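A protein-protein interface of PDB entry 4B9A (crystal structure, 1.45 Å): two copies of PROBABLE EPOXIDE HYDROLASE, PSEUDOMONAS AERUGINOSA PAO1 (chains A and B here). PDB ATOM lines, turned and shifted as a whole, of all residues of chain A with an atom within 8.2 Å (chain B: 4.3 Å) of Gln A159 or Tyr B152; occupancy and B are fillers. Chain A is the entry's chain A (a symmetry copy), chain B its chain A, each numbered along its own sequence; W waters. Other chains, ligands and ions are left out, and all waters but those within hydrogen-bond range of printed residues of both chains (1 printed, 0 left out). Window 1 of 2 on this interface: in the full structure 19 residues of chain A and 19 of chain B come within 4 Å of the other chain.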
ATOM      1  N   ALA A 148     -11.943 -16.355 -18.220  1.00  0.00           N
ATOM      2  CA  ALA A 148     -12.439 -16.009 -16.892  1.00  0.00           C
ATOM      3  C   ALA A 148     -12.108 -14.550 -16.523  1.00  0.00           C
ATOM      4  O   ALA A 148     -12.873 -13.933 -15.788  1.00  0.00           O
ATOM      5  CB  ALA A 148     -11.980 -17.021 -15.868  1.00  0.00           C
ATOM      6  N   LEU A 149     -10.972 -14.033 -16.976  1.00  0.00           N
ATOM      7  CA  LEU A 149     -10.710 -12.608 -16.780  1.00  0.00           C
ATOM      8  C   LEU A 149     -11.651 -11.724 -17.602  1.00  0.00           C
ATOM      9  O   LEU A 149     -12.147 -10.715 -17.117  1.00  0.00           O
ATOM     10  CB  LEU A 149      -9.268 -12.274 -17.081  1.00  0.00           C
ATOM     11  CG  LEU A 149      -8.283 -12.847 -16.081  1.00  0.00           C
ATOM     12  CD1 LEU A 149      -6.847 -12.903 -16.634  1.00  0.00           C
ATOM     13  CD2 LEU A 149      -8.360 -12.113 -14.734  1.00  0.00           C
ATOM     14  N   TYR A 152     -15.418 -12.189 -16.277  1.00  0.00           N
ATOM     15  CA  TYR A 152     -15.362 -12.391 -14.825  1.00  0.00           C
ATOM     16  C   TYR A 152     -16.755 -12.441 -14.222  1.00  0.00           C
ATOM     17  O   TYR A 152     -16.958 -13.093 -13.182  1.00  0.00           O
ATOM     18  CB  TYR A 152     -14.489 -11.320 -14.139  1.00  0.00           C
ATOM     19  CG  TYR A 152     -15.230 -10.036 -13.940  1.00  0.00           C
ATOM     20  CD1 TYR A 152     -15.455  -9.150 -14.985  1.00  0.00           C
ATOM     21  CD2 TYR A 152     -15.847  -9.761 -12.724  1.00  0.00           C
ATOM     22  CE1 TYR A 152     -16.297  -8.046 -14.825  1.00  0.00           C
ATOM     23  CE2 TYR A 152     -16.671  -8.665 -12.576  1.00  0.00           C
ATOM     24  CZ  TYR A 152     -16.883  -7.802 -13.608  1.00  0.00           C
ATOM     25  OH  TYR A 152     -17.734  -6.733 -13.422  1.00  0.00           O
ATOM     26  N   HIS A 153     -17.692 -11.702 -14.826  1.00  0.00           N
ATOM     27  CA  HIS A 153     -19.029 -11.624 -14.295  1.00  0.00           C
ATOM     28  C   HIS A 153     -19.778 -12.953 -14.367  1.00  0.00           C
ATOM     29  O   HIS A 153     -20.696 -13.160 -13.583  1.00  0.00           O
ATOM     30  CB  HIS A 153     -19.829 -10.497 -14.964  1.00  0.00           C
ATOM     31  CG  HIS A 153     -20.080 -10.720 -16.412  1.00  0.00           C
ATOM     32  ND1 HIS A 153     -19.065 -10.760 -17.349  1.00  0.00           N
ATOM     33  CD2 HIS A 153     -21.232 -10.878 -17.098  1.00  0.00           C
ATOM     34  CE1 HIS A 153     -19.583 -10.982 -18.538  1.00  0.00           C
ATOM     35  NE2 HIS A 153     -20.894 -11.072 -18.417  1.00  0.00           N
ATOM     36  N   TRP A 154     -19.414 -13.827 -15.282  1.00  0.00           N
ATOM     37  CA  TRP A 154     -20.025 -15.141 -15.325  1.00  0.00           C
ATOM     38  C   TRP A 154     -19.797 -15.881 -14.024  1.00  0.00           C
ATOM     39  O   TRP A 154     -20.597 -16.720 -13.595  1.00  0.00           O
ATOM     40  CB  TRP A 154     -19.453 -15.989 -16.451  1.00  0.00           C
ATOM     41  CG  TRP A 154     -19.956 -15.649 -17.820  1.00  0.00           C
ATOM     42  CD1 TRP A 154     -20.316 -14.425 -18.305  1.00  0.00           C
ATOM     43  CD2 TRP A 154     -20.202 -16.573 -18.854  1.00  0.00           C
ATOM     44  NE1 TRP A 154     -20.740 -14.541 -19.612  1.00  0.00           N
ATOM     45  CE2 TRP A 154     -20.722 -15.869 -19.946  1.00  0.00           C
ATOM     46  CE3 TRP A 154     -20.053 -17.957 -18.954  1.00  0.00           C
ATOM     47  CZ2 TRP A 154     -21.045 -16.510 -21.152  1.00  0.00           C
ATOM     48  CZ3 TRP A 154     -20.419 -18.574 -20.139  1.00  0.00           C
ATOM     49  CH2 TRP A 154     -20.937 -17.851 -21.199  1.00  0.00           C
ATOM     50  N   PHE A 155     -18.645 -15.597 -13.396  1.00  0.00           N
ATOM     51  CA  PHE A 155     -18.248 -16.235 -12.146  1.00  0.00           C
ATOM     52  C   PHE A 155     -18.735 -15.488 -10.930  1.00  0.00           C
ATOM     53  O   PHE A 155     -19.201 -16.102  -9.976  1.00  0.00           O
ATOM     54  CB  PHE A 155     -16.730 -16.488 -12.184  1.00  0.00           C
ATOM     55  CG  PHE A 155     -16.378 -17.320 -13.401  1.00  0.00           C
ATOM     56  CD1 PHE A 155     -16.585 -18.702 -13.418  1.00  0.00           C
ATOM     57  CD2 PHE A 155     -15.922 -16.693 -14.570  1.00  0.00           C
ATOM     58  CE1 PHE A 155     -16.368 -19.447 -14.559  1.00  0.00           C
ATOM     59  CE2 PHE A 155     -15.698 -17.449 -15.725  1.00  0.00           C
ATOM     60  CZ  PHE A 155     -15.948 -18.831 -15.720  1.00  0.00           C
ATOM     61  N   LEU A 156     -18.665 -14.162 -10.984  1.00  0.00           N
ATOM     62  CA  LEU A 156     -19.140 -13.334  -9.864  1.00  0.00           C
ATOM     63  C   LEU A 156     -20.675 -13.547  -9.686  1.00  0.00           C
ATOM     64  O   LEU A 156     -21.175 -13.794  -8.573  1.00  0.00           O
ATOM     65  CB  LEU A 156     -18.832 -11.889 -10.072  1.00  0.00           C
ATOM     66  CG  LEU A 156     -19.537 -10.935  -9.089  1.00  0.00           C
ATOM     67  CD1 LEU A 156     -19.139 -11.181  -7.666  1.00  0.00           C
ATOM     68  CD2 LEU A 156     -19.274  -9.496  -9.498  1.00  0.00           C
ATOM     69  N   LEU A 157     -21.427 -13.360 -10.775  1.00  0.00           N
ATOM     70  CA  LEU A 157     -22.892 -13.329 -10.694  1.00  0.00           C
ATOM     71  C   LEU A 157     -23.482 -14.681 -10.347  1.00  0.00           C
ATOM     72  O   LEU A 157     -24.622 -14.735  -9.853  1.00  0.00           O
ATOM     73  CB  LEU A 157     -23.496 -12.766 -11.973  1.00  0.00           C
ATOM     74  CG  LEU A 157     -23.104 -11.350 -12.389  1.00  0.00           C
ATOM     75  CD1 LEU A 157     -23.663 -10.987 -13.780  1.00  0.00           C
ATOM     76  CD2 LEU A 157     -23.447 -10.359 -11.306  1.00  0.00           C
ATOM     77  N   ALA A 158     -22.689 -15.759 -10.551  1.00  0.00           N
ATOM     78  CA  ALA A 158     -23.111 -17.112 -10.243  1.00  0.00           C
ATOM     79  C   ALA A 158     -22.807 -17.549  -8.794  1.00  0.00           C
ATOM     80  O   ALA A 158     -23.124 -18.669  -8.358  1.00  0.00           O
ATOM     81  CB  ALA A 158     -22.496 -18.099 -11.236  1.00  0.00           C
ATOM     82  N   GLN A 159     -22.127 -16.691  -8.016  1.00  0.00           N
ATOM     83  CA  GLN A 159     -21.834 -17.051  -6.627  1.00  0.00           C
ATOM     84  C   GLN A 159     -23.128 -17.157  -5.840  1.00  0.00           C
ATOM     85  O   GLN A 159     -24.141 -16.550  -6.230  1.00  0.00           O
ATOM     86  CB  GLN A 159     -20.880 -16.057  -6.010  1.00  0.00           C
ATOM     87  CG  GLN A 159     -19.529 -15.990  -6.684  1.00  0.00           C
ATOM     88  CD  GLN A 159     -18.864 -17.368  -6.667  1.00  0.00           C
ATOM     89  OE1 GLN A 159     -18.738 -18.020  -5.609  1.00  0.00           O
ATOM     90  NE2 GLN A 159     -18.453 -17.834  -7.841  1.00  0.00           N
ATOM     91  N   PRO A 160     -23.097 -17.885  -4.747  1.00  0.00           N
ATOM     92  CA  PRO A 160     -24.340 -18.079  -4.063  1.00  0.00           C
ATOM     93  C   PRO A 160     -24.988 -16.789  -3.508  1.00  0.00           C
ATOM     94  O   PRO A 160     -24.301 -15.821  -3.138  1.00  0.00           O
ATOM     95  CB  PRO A 160     -23.991 -19.039  -2.922  1.00  0.00           C
ATOM     96  CG  PRO A 160     -22.734 -19.713  -3.358  1.00  0.00           C
ATOM     97  CD  PRO A 160     -22.020 -18.736  -4.250  1.00  0.00           C
ATOM     98  N   TYR A 161     -26.311 -16.836  -3.429  1.00  0.00           N
ATOM     99  CA  TYR A 161     -27.084 -15.735  -2.875  1.00  0.00           C
ATOM    100  C   TYR A 161     -26.545 -15.420  -1.478  1.00  0.00           C
ATOM    101  O   TYR A 161     -26.333 -16.340  -0.674  1.00  0.00           O
ATOM    102  CB  TYR A 161     -28.535 -16.125  -2.810  1.00  0.00           C
ATOM    103  CG  TYR A 161     -29.416 -15.070  -2.258  1.00  0.00           C
ATOM    104  CD1 TYR A 161     -29.791 -13.977  -3.006  1.00  0.00           C
ATOM    105  CD2 TYR A 161     -29.863 -15.128  -0.954  1.00  0.00           C
ATOM    106  CE1 TYR A 161     -30.621 -13.003  -2.497  1.00  0.00           C
ATOM    107  CE2 TYR A 161     -30.677 -14.136  -0.424  1.00  0.00           C
ATOM    108  CZ  TYR A 161     -31.093 -13.091  -1.212  1.00  0.00           C
ATOM    109  OH  TYR A 161     -31.876 -12.057  -0.709  1.00  0.00           O
ATOM    110  N   ASP A 162     -26.312 -14.162  -1.103  1.00  0.00           N
ATOM    111  CA  ASP A 162     -26.603 -12.915  -1.835  1.00  0.00           C
ATOM    112  C   ASP A 162     -25.289 -12.160  -2.128  1.00  0.00           C
ATOM    113  O   ASP A 162     -25.304 -10.938  -2.151  1.00  0.00           O
ATOM    114  CB  ASP A 162     -27.564 -12.039  -1.011  1.00  0.00           C
ATOM    115  CG  ASP A 162     -26.989 -11.587   0.330  1.00  0.00           C
ATOM    116  OD1 ASP A 162     -25.994 -12.160   0.818  1.00  0.00           O
ATOM    117  OD2 ASP A 162     -27.624 -10.702   0.932  1.00  0.00           O
ATOM    118  N   LEU A 163     -24.187 -12.874  -2.320  1.00  0.00           N
ATOM    119  CA  LEU A 163     -22.881 -12.226  -2.549  1.00  0.00           C
ATOM    120  C   LEU A 163     -22.908 -11.221  -3.708  1.00  0.00           C
ATOM    121  O   LEU A 163     -22.630 -10.040  -3.517  1.00  0.00           O
ATOM    122  CB  LEU A 163     -21.765 -13.287  -2.663  1.00  0.00           C
ATOM    123  CG  LEU A 163     -20.309 -12.828  -2.829  1.00  0.00           C
ATOM    124  CD1 LEU A 163     -20.006 -12.410  -4.259  1.00  0.00           C
ATOM    125  CD2 LEU A 163     -20.010 -11.699  -1.825  1.00  0.00           C
ATOM    126  N   PRO A 164     -23.283 -11.687  -4.926  1.00  0.00           N
ATOM    127  CA  PRO A 164     -23.184 -10.723  -6.025  1.00  0.00           C
ATOM    128  C   PRO A 164     -24.242  -9.639  -5.914  1.00  0.00           C
ATOM    129  O   PRO A 164     -23.959  -8.489  -6.239  1.00  0.00           O
ATOM    130  CB  PRO A 164     -23.347 -11.589  -7.269  1.00  0.00           C
ATOM    131  CG  PRO A 164     -24.088 -12.805  -6.839  1.00  0.00           C
ATOM    132  CD  PRO A 164     -23.537 -13.047  -5.431  1.00  0.00           C
ATOM    133  N   GLU A 165     -25.418  -9.978  -5.377  1.00  0.00           N
ATOM    134  CA  GLU A 165     -26.453  -8.944  -5.165  1.00  0.00           C
ATOM    135  C   GLU A 165     -25.918  -7.847  -4.275  1.00  0.00           C
ATOM    136  O   GLU A 165     -26.154  -6.673  -4.530  1.00  0.00           O
ATOM    137  CB  GLU A 165     -27.716  -9.538  -4.538  1.00  0.00           C
ATOM    138  CG  GLU A 165     -28.556 -10.419  -5.441  1.00  0.00           C
ATOM    139  CD  GLU A 165     -28.160 -11.894  -5.508  1.00  0.00           C
ATOM    140  OE1 GLU A 165     -27.046 -12.307  -5.073  1.00  0.00           O
ATOM    141  OE2 GLU A 165     -28.999 -12.664  -6.075  1.00  0.00           O
ATOM    142  N   LEU A 167     -22.790  -6.922  -3.873  1.00  0.00           N
ATOM    143  CA  LEU A 167     -21.707  -6.180  -4.515  1.00  0.00           C
ATOM    144  C   LEU A 167     -22.260  -5.267  -5.648  1.00  0.00           C
ATOM    145  O   LEU A 167     -21.912  -4.079  -5.747  1.00  0.00           O
ATOM    146  CB  LEU A 167     -20.637  -7.113  -5.052  1.00  0.00           C
ATOM    147  CG  LEU A 167     -19.874  -7.903  -4.009  1.00  0.00           C
ATOM    148  CD1 LEU A 167     -18.703  -8.633  -4.666  1.00  0.00           C
ATOM    149  CD2 LEU A 167     -19.408  -7.089  -2.854  1.00  0.00           C
ATOM    150  N   CYS A 212     -28.687 -12.279 -11.439  1.00  0.00           N
ATOM    151  CA  CYS A 212     -27.797 -13.253 -10.776  1.00  0.00           C
ATOM    152  C   CYS A 212     -28.353 -14.661 -10.940  1.00  0.00           C
ATOM    153  O   CYS A 212     -27.597 -15.624 -11.167  1.00  0.00           O
ATOM    154  CB  CYS A 212     -27.581 -12.934  -9.304  1.00  0.00           C
ATOM    155  SG  CYS A 212     -26.687 -11.354  -9.070  1.00  0.00           S
ATOM    156  N   GLU A 213     -29.677 -14.799 -10.827  1.00  0.00           N
ATOM    157  CA  GLU A 213     -30.262 -16.127 -10.943  1.00  0.00           C
ATOM    158  C   GLU A 213     -30.061 -16.736 -12.339  1.00  0.00           C
ATOM    159  O   GLU A 213     -29.886 -17.938 -12.453  1.00  0.00           O
ATOM    160  CB  GLU A 213     -31.753 -16.105 -10.611  1.00  0.00           C
ATOM    161  CG  GLU A 213     -32.032 -15.918  -9.113  1.00  0.00           C
ATOM    162  CD  GLU A 213     -31.635 -17.121  -8.297  1.00  0.00           C
ATOM    163  OE1 GLU A 213     -32.154 -18.234  -8.551  1.00  0.00           O
ATOM    164  OE2 GLU A 213     -30.781 -17.024  -7.414  1.00  0.00           O
ATOM    165  N   TYR A 215     -27.447 -16.168 -14.243  1.00  0.00           N
ATOM    166  CA  TYR A 215     -26.064 -16.616 -14.246  1.00  0.00           C
ATOM    167  C   TYR A 215     -25.845 -17.892 -13.416  1.00  0.00           C
ATOM    168  O   TYR A 215     -25.005 -18.713 -13.748  1.00  0.00           O
ATOM    169  CB  TYR A 215     -25.104 -15.477 -13.906  1.00  0.00           C
ATOM    170  CG  TYR A 215     -24.920 -14.513 -15.042  1.00  0.00           C
ATOM    171  CD1 TYR A 215     -25.793 -13.472 -15.264  1.00  0.00           C
ATOM    172  CD2 TYR A 215     -23.946 -14.708 -15.975  1.00  0.00           C
ATOM    173  CE1 TYR A 215     -25.657 -12.648 -16.352  1.00  0.00           C
ATOM    174  CE2 TYR A 215     -23.799 -13.845 -17.083  1.00  0.00           C
ATOM    175  CZ  TYR A 215     -24.696 -12.814 -17.272  1.00  0.00           C
ATOM    176  OH  TYR A 215     -24.546 -11.966 -18.358  1.00  0.00           O
ATOM    177  N   ARG A 216     -26.580 -17.996 -12.305  1.00  0.00           N
ATOM    178  CA  ARG A 216     -26.557 -19.233 -11.517  1.00  0.00           C
ATOM    179  C   ARG A 216     -27.093 -20.436 -12.294  1.00  0.00           C
ATOM    180  O   ARG A 216     -26.537 -21.533 -12.253  1.00  0.00           O
ATOM    181  CB  ARG A 216     -27.298 -19.089 -10.179  1.00  0.00           C
ATOM    182  CG  ARG A 216     -26.675 -18.076  -9.228  1.00  0.00           C
ATOM    183  CD  ARG A 216     -27.530 -17.828  -7.979  1.00  0.00           C
ATOM    184  NE  ARG A 216     -26.867 -16.908  -7.110  1.00  0.00           N
ATOM    185  CZ  ARG A 216     -27.306 -15.715  -6.745  1.00  0.00           C
ATOM    186  NH1 ARG A 216     -28.557 -15.317  -6.935  1.00  0.00           N
ATOM    187  NH2 ARG A 216     -26.484 -14.889  -6.126  1.00  0.00           N
ATOM    188  N   VAL A 219     -24.602 -21.932 -14.840  1.00  0.00           N
ATOM    189  CA  VAL A 219     -23.680 -22.891 -14.251  1.00  0.00           C
ATOM    190  C   VAL A 219     -24.321 -24.245 -14.079  1.00  0.00           C
ATOM    191  O   VAL A 219     -23.661 -25.275 -14.322  1.00  0.00           O
ATOM    192  CB  VAL A 219     -23.184 -22.351 -12.885  1.00  0.00           C
ATOM    193  CG1 VAL A 219     -22.500 -23.431 -12.076  1.00  0.00           C
ATOM    194  CG2 VAL A 219     -22.230 -21.163 -13.113  1.00  0.00           C
ATOM    195  N   ALA B 148     -12.683 -21.435 -11.560  1.00  0.00           N
ATOM    196  CA  ALA B 148     -13.089 -20.037 -11.657  1.00  0.00           C
ATOM    197  C   ALA B 148     -14.327 -19.742 -10.789  1.00  0.00           C
ATOM    198  O   ALA B 148     -14.459 -18.624 -10.301  1.00  0.00           O
ATOM    199  CB  ALA B 148     -13.239 -19.622 -13.103  1.00  0.00           C
ATOM    200  N   LEU B 149     -15.235 -20.701 -10.648  1.00  0.00           N
ATOM    201  CA  LEU B 149     -16.333 -20.507  -9.702  1.00  0.00           C
ATOM    202  C   LEU B 149     -15.856 -20.495  -8.248  1.00  0.00           C
ATOM    203  O   LEU B 149     -16.301 -19.683  -7.449  1.00  0.00           O
ATOM    204  CB  LEU B 149     -17.410 -21.548  -9.900  1.00  0.00           C
ATOM    205  CG  LEU B 149     -18.174 -21.402 -11.202  1.00  0.00           C
ATOM    206  CD1 LEU B 149     -18.914 -22.693 -11.598  1.00  0.00           C
ATOM    207  CD2 LEU B 149     -19.107 -20.182 -11.170  1.00  0.00           C
ATOM    208  N   ASN B 150     -14.970 -21.449  -7.901  1.00  0.00           N
ATOM    209  CA  ASN B 150     -14.513 -21.566  -6.516  1.00  0.00           C
ATOM    210  C   ASN B 150     -13.650 -20.350  -6.133  1.00  0.00           C
ATOM    211  O   ASN B 150     -13.779 -19.799  -5.053  1.00  0.00           O
ATOM    212  CB  ASN B 150     -13.708 -22.881  -6.268  1.00  0.00           C
ATOM    213  CG  ASN B 150     -14.587 -24.146  -6.281  1.00  0.00           C
ATOM    214  OD1 ASN B 150     -15.790 -24.051  -6.326  1.00  0.00           O
ATOM    215  ND2 ASN B 150     -13.968 -25.316  -6.246  1.00  0.00           N
ATOM    216  N   ALA B 151     -12.772 -19.946  -7.052  1.00  0.00           N
ATOM    217  CA  ALA B 151     -11.798 -18.875  -6.842  1.00  0.00           C
ATOM    218  C   ALA B 151     -12.204 -17.625  -7.650  1.00  0.00           C
ATOM    219  O   ALA B 151     -11.372 -16.992  -8.322  1.00  0.00           O
ATOM    220  CB  ALA B 151     -10.390 -19.348  -7.175  1.00  0.00           C
ATOM    221  N   TYR B 152     -13.505 -17.291  -7.641  1.00  0.00           N
ATOM    222  CA  TYR B 152     -14.026 -16.190  -8.459  1.00  0.00           C
ATOM    223  C   TYR B 152     -13.274 -14.898  -8.187  1.00  0.00           C
ATOM    224  O   TYR B 152     -13.181 -14.035  -9.078  1.00  0.00           O
ATOM    225  CB  TYR B 152     -15.545 -16.010  -8.263  1.00  0.00           C
ATOM    226  CG  TYR B 152     -15.863 -15.246  -7.018  1.00  0.00           C
ATOM    227  CD1 TYR B 152     -15.793 -15.831  -5.760  1.00  0.00           C
ATOM    228  CD2 TYR B 152     -16.097 -13.876  -7.074  1.00  0.00           C
ATOM    229  CE1 TYR B 152     -15.920 -15.063  -4.600  1.00  0.00           C
ATOM    230  CE2 TYR B 152     -16.226 -13.128  -5.921  1.00  0.00           C
ATOM    231  CZ  TYR B 152     -16.157 -13.714  -4.693  1.00  0.00           C
ATOM    232  OH  TYR B 152     -16.267 -12.925  -3.568  1.00  0.00           O
ATOM    233  N   HIS B 153     -12.805 -14.734  -6.945  1.00  0.00           N
ATOM    234  CA  HIS B 153     -12.138 -13.515  -6.562  1.00  0.00           C
ATOM    235  C   HIS B 153     -10.808 -13.311  -7.283  1.00  0.00           C
ATOM    236  O   HIS B 153     -10.370 -12.174  -7.412  1.00  0.00           O
ATOM    237  CB  HIS B 153     -11.964 -13.431  -5.039  1.00  0.00           C
ATOM    238  CG  HIS B 153     -11.060 -14.471  -4.481  1.00  0.00           C
ATOM    239  ND1 HIS B 153     -11.357 -15.820  -4.524  1.00  0.00           N
ATOM    240  CD2 HIS B 153      -9.881 -14.366  -3.833  1.00  0.00           C
ATOM    241  CE1 HIS B 153     -10.375 -16.497  -3.969  1.00  0.00           C
ATOM    242  NE2 HIS B 153      -9.458 -15.644  -3.551  1.00  0.00           N
ATOM    243  N   TRP B 154     -10.171 -14.373  -7.733  1.00  0.00           N
ATOM    244  CA  TRP B 154      -8.958 -14.224  -8.512  1.00  0.00           C
ATOM    245  C   TRP B 154      -9.220 -13.416  -9.765  1.00  0.00           C
ATOM    246  O   TRP B 154      -8.349 -12.717 -10.293  1.00  0.00           O
ATOM    247  CB  TRP B 154      -8.393 -15.572  -8.935  1.00  0.00           C
ATOM    248  CG  TRP B 154      -7.677 -16.326  -7.858  1.00  0.00           C
ATOM    249  CD1 TRP B 154      -7.943 -16.340  -6.520  1.00  0.00           C
ATOM    250  CD2 TRP B 154      -6.536 -17.132  -8.044  1.00  0.00           C
ATOM    251  NE1 TRP B 154      -7.038 -17.151  -5.867  1.00  0.00           N
ATOM    252  CE2 TRP B 154      -6.135 -17.606  -6.790  1.00  0.00           C
ATOM    253  CE3 TRP B 154      -5.788 -17.483  -9.168  1.00  0.00           C
ATOM    254  CZ2 TRP B 154      -5.036 -18.466  -6.643  1.00  0.00           C
ATOM    255  CZ3 TRP B 154      -4.682 -18.299  -8.993  1.00  0.00           C
ATOM    256  CH2 TRP B 154      -4.306 -18.746  -7.739  1.00  0.00           C
ATOM    257  N   PHE B 155     -10.449 -13.551 -10.288  1.00  0.00           N
ATOM    258  CA  PHE B 155     -10.869 -12.870 -11.508  1.00  0.00           C
ATOM    259  C   PHE B 155     -11.470 -11.513 -11.240  1.00  0.00           C
ATOM    260  O   PHE B 155     -11.179 -10.559 -11.954  1.00  0.00           O
ATOM    261  CB  PHE B 155     -11.763 -13.824 -12.321  1.00  0.00           C
ATOM    262  CG  PHE B 155     -11.018 -15.113 -12.601  1.00  0.00           C
ATOM    263  CD1 PHE B 155     -10.057 -15.190 -13.612  1.00  0.00           C
ATOM    264  CD2 PHE B 155     -11.221 -16.231 -11.778  1.00  0.00           C
ATOM    265  CE1 PHE B 155      -9.300 -16.328 -13.800  1.00  0.00           C
ATOM    266  CE2 PHE B 155     -10.456 -17.386 -11.971  1.00  0.00           C
ATOM    267  CZ  PHE B 155      -9.474 -17.420 -12.974  1.00  0.00           C
ATOM    268  N   LEU B 156     -12.273 -11.421 -10.186  1.00  0.00           N
ATOM    269  CA  LEU B 156     -12.890 -10.137  -9.816  1.00  0.00           C
ATOM    270  C   LEU B 156     -11.769  -9.124  -9.429  1.00  0.00           C
ATOM    271  O   LEU B 156     -11.735  -7.973  -9.906  1.00  0.00           O
ATOM    272  CB  LEU B 156     -13.865 -10.290  -8.698  1.00  0.00           C
ATOM    273  CG  LEU B 156     -14.339  -8.965  -8.072  1.00  0.00           C
ATOM    274  CD1 LEU B 156     -15.060  -8.093  -9.054  1.00  0.00           C
ATOM    275  CD2 LEU B 156     -15.197  -9.254  -6.853  1.00  0.00           C
ATOM    276  N   PHE B 175     -18.035  -7.954   3.343  1.00  0.00           N
ATOM    277  CA  PHE B 175     -17.282  -8.741   2.369  1.00  0.00           C
ATOM    278  C   PHE B 175     -16.129  -9.474   3.038  1.00  0.00           C
ATOM    279  O   PHE B 175     -15.873 -10.663   2.744  1.00  0.00           O
ATOM    280  CB  PHE B 175     -16.781  -7.850   1.225  1.00  0.00           C
ATOM    281  CG  PHE B 175     -16.026  -8.616   0.185  1.00  0.00           C
ATOM    282  CD1 PHE B 175     -16.674  -9.340  -0.782  1.00  0.00           C
ATOM    283  CD2 PHE B 175     -14.666  -8.692   0.243  1.00  0.00           C
ATOM    284  CE1 PHE B 175     -15.971 -10.086  -1.701  1.00  0.00           C
ATOM    285  CE2 PHE B 175     -13.960  -9.440  -0.667  1.00  0.00           C
ATOM    286  CZ  PHE B 175     -14.620 -10.115  -1.643  1.00  0.00           C
ATOM    287  N   ARG B 182     -15.948 -18.182   4.273  1.00  0.00           N
ATOM    288  CA  ARG B 182     -15.865 -19.075   3.134  1.00  0.00           C
ATOM    289  C   ARG B 182     -14.516 -19.790   3.086  1.00  0.00           C
ATOM    290  O   ARG B 182     -14.432 -20.990   2.842  1.00  0.00           O
ATOM    291  CB  ARG B 182     -16.114 -18.255   1.872  1.00  0.00           C
ATOM    292  CG  ARG B 182     -15.963 -19.003   0.563  1.00  0.00           C
ATOM    293  CD  ARG B 182     -16.590 -18.234  -0.573  1.00  0.00           C
ATOM    294  NE  ARG B 182     -16.263 -18.879  -1.838  1.00  0.00           N
ATOM    295  CZ  ARG B 182     -16.904 -18.657  -2.960  1.00  0.00           C
ATOM    296  NH1 ARG B 182     -17.933 -17.826  -2.985  1.00  0.00           N
ATOM    297  NH2 ARG B 182     -16.500 -19.269  -4.080  1.00  0.00           N
HETATM  298  O   HOH W   1     -15.424 -12.879 -10.646  1.00  0.00           O
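O of Asn B150 is in hydrogen-bond range of NH2 of Arg B182. NE2 of Gln A159 lies within hydrogen-bond range of O of Phe A155 (2.8 Å). O of Leu B149 lies within hydrogen-bond range of NH2 of Arg B182 (3.4 Å). NH2 of Arg A216 lies within hydrogen-bond range of O of Gln A159, 2.9 Å away.
Water W1 lies within hydrogen-bond range of the backbone carbonyl oxygen of Tyr B152 (3.0 Å) and the backbone carbonyl oxygen of Tyr A152 (3.0 Å).
The side-chain amide nitrogen of Gln A159 lies within hydrogen-bond range of the backbone carbonyl oxygen of Leu B149, 2.9 Å away. OE1 of Gln A159 is in hydrogen-bond range of NH1 of Arg B182.
Gln A159 touches just these residues of chain B: Leu B149 (2.9 Å), Tyr B152 (3.5 Å) and Arg B182 (2.8 Å). Of the printed residues of chain B, Leu A163 touches Tyr B152 (3.8 Å). Printed residues of chain A within 4 Å of Ala B148: Ala A148 and Phe A155. No residue of chain A comes within 4 Å of Ala B151. Of the printed residues of chain A, Tyr B152 touches Leu A156, Gln A159 and Leu A163. The nearest printed residue of chain A that does not touch Tyr B152 is Phe A155 (4.04 Å). The nearest printed residue of chain A that does not touch Phe B155 is Tyr A152 (4.04 Å).
Of the 11 printed residues of chain B, 6 touch a printed residue of chain A. Among the printed residues, 13 pairs touch across the chains. Among the printed residues, no Asp or Glu carboxylate lies within 4 Å of a Lys or Arg side-chain nitrogen of the other chain.
Ala B148 touches its own counterpart, Ala A148. Ala A148 touches Phe B155, and with the chains exchanged Phe A155 touches Ala B148. Leu A149 touches Phe B155, and with the chains exchanged Phe A155 touches Leu B149. Tyr A152 touches Leu B156, and with the chains exchanged Leu A156 touches Tyr B152. Positions printed for both chains: 148, 149, 152, 153, 154, 155 and 156. Of the 13 pairs that touch across the chains among the printed residues, 7 have their exchanged pair printed and touching as well.
Among the printed residues, pairs that only touch across the chains: Ala A148 with Ala B148 (3.999 Å), Ala A148 with Phe B155 (3.5 Å), Leu A149 with Phe B155 (3.7 Å), Tyr A152 with Leu B156 (3.9 Å), Phe A155 with Ala B148 (3.5 Å), Phe A155 with Leu B149 (3.7 Å), Leu A156 with Tyr B152 (3.9 Å), Ala A158 with Leu B149 (3.98 Å), Gln A159 with Tyr B152 (3.5 Å), Leu A163 with Tyr B152 (3.8 Å) and Val A219 with Leu B149 (3.7 Å).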
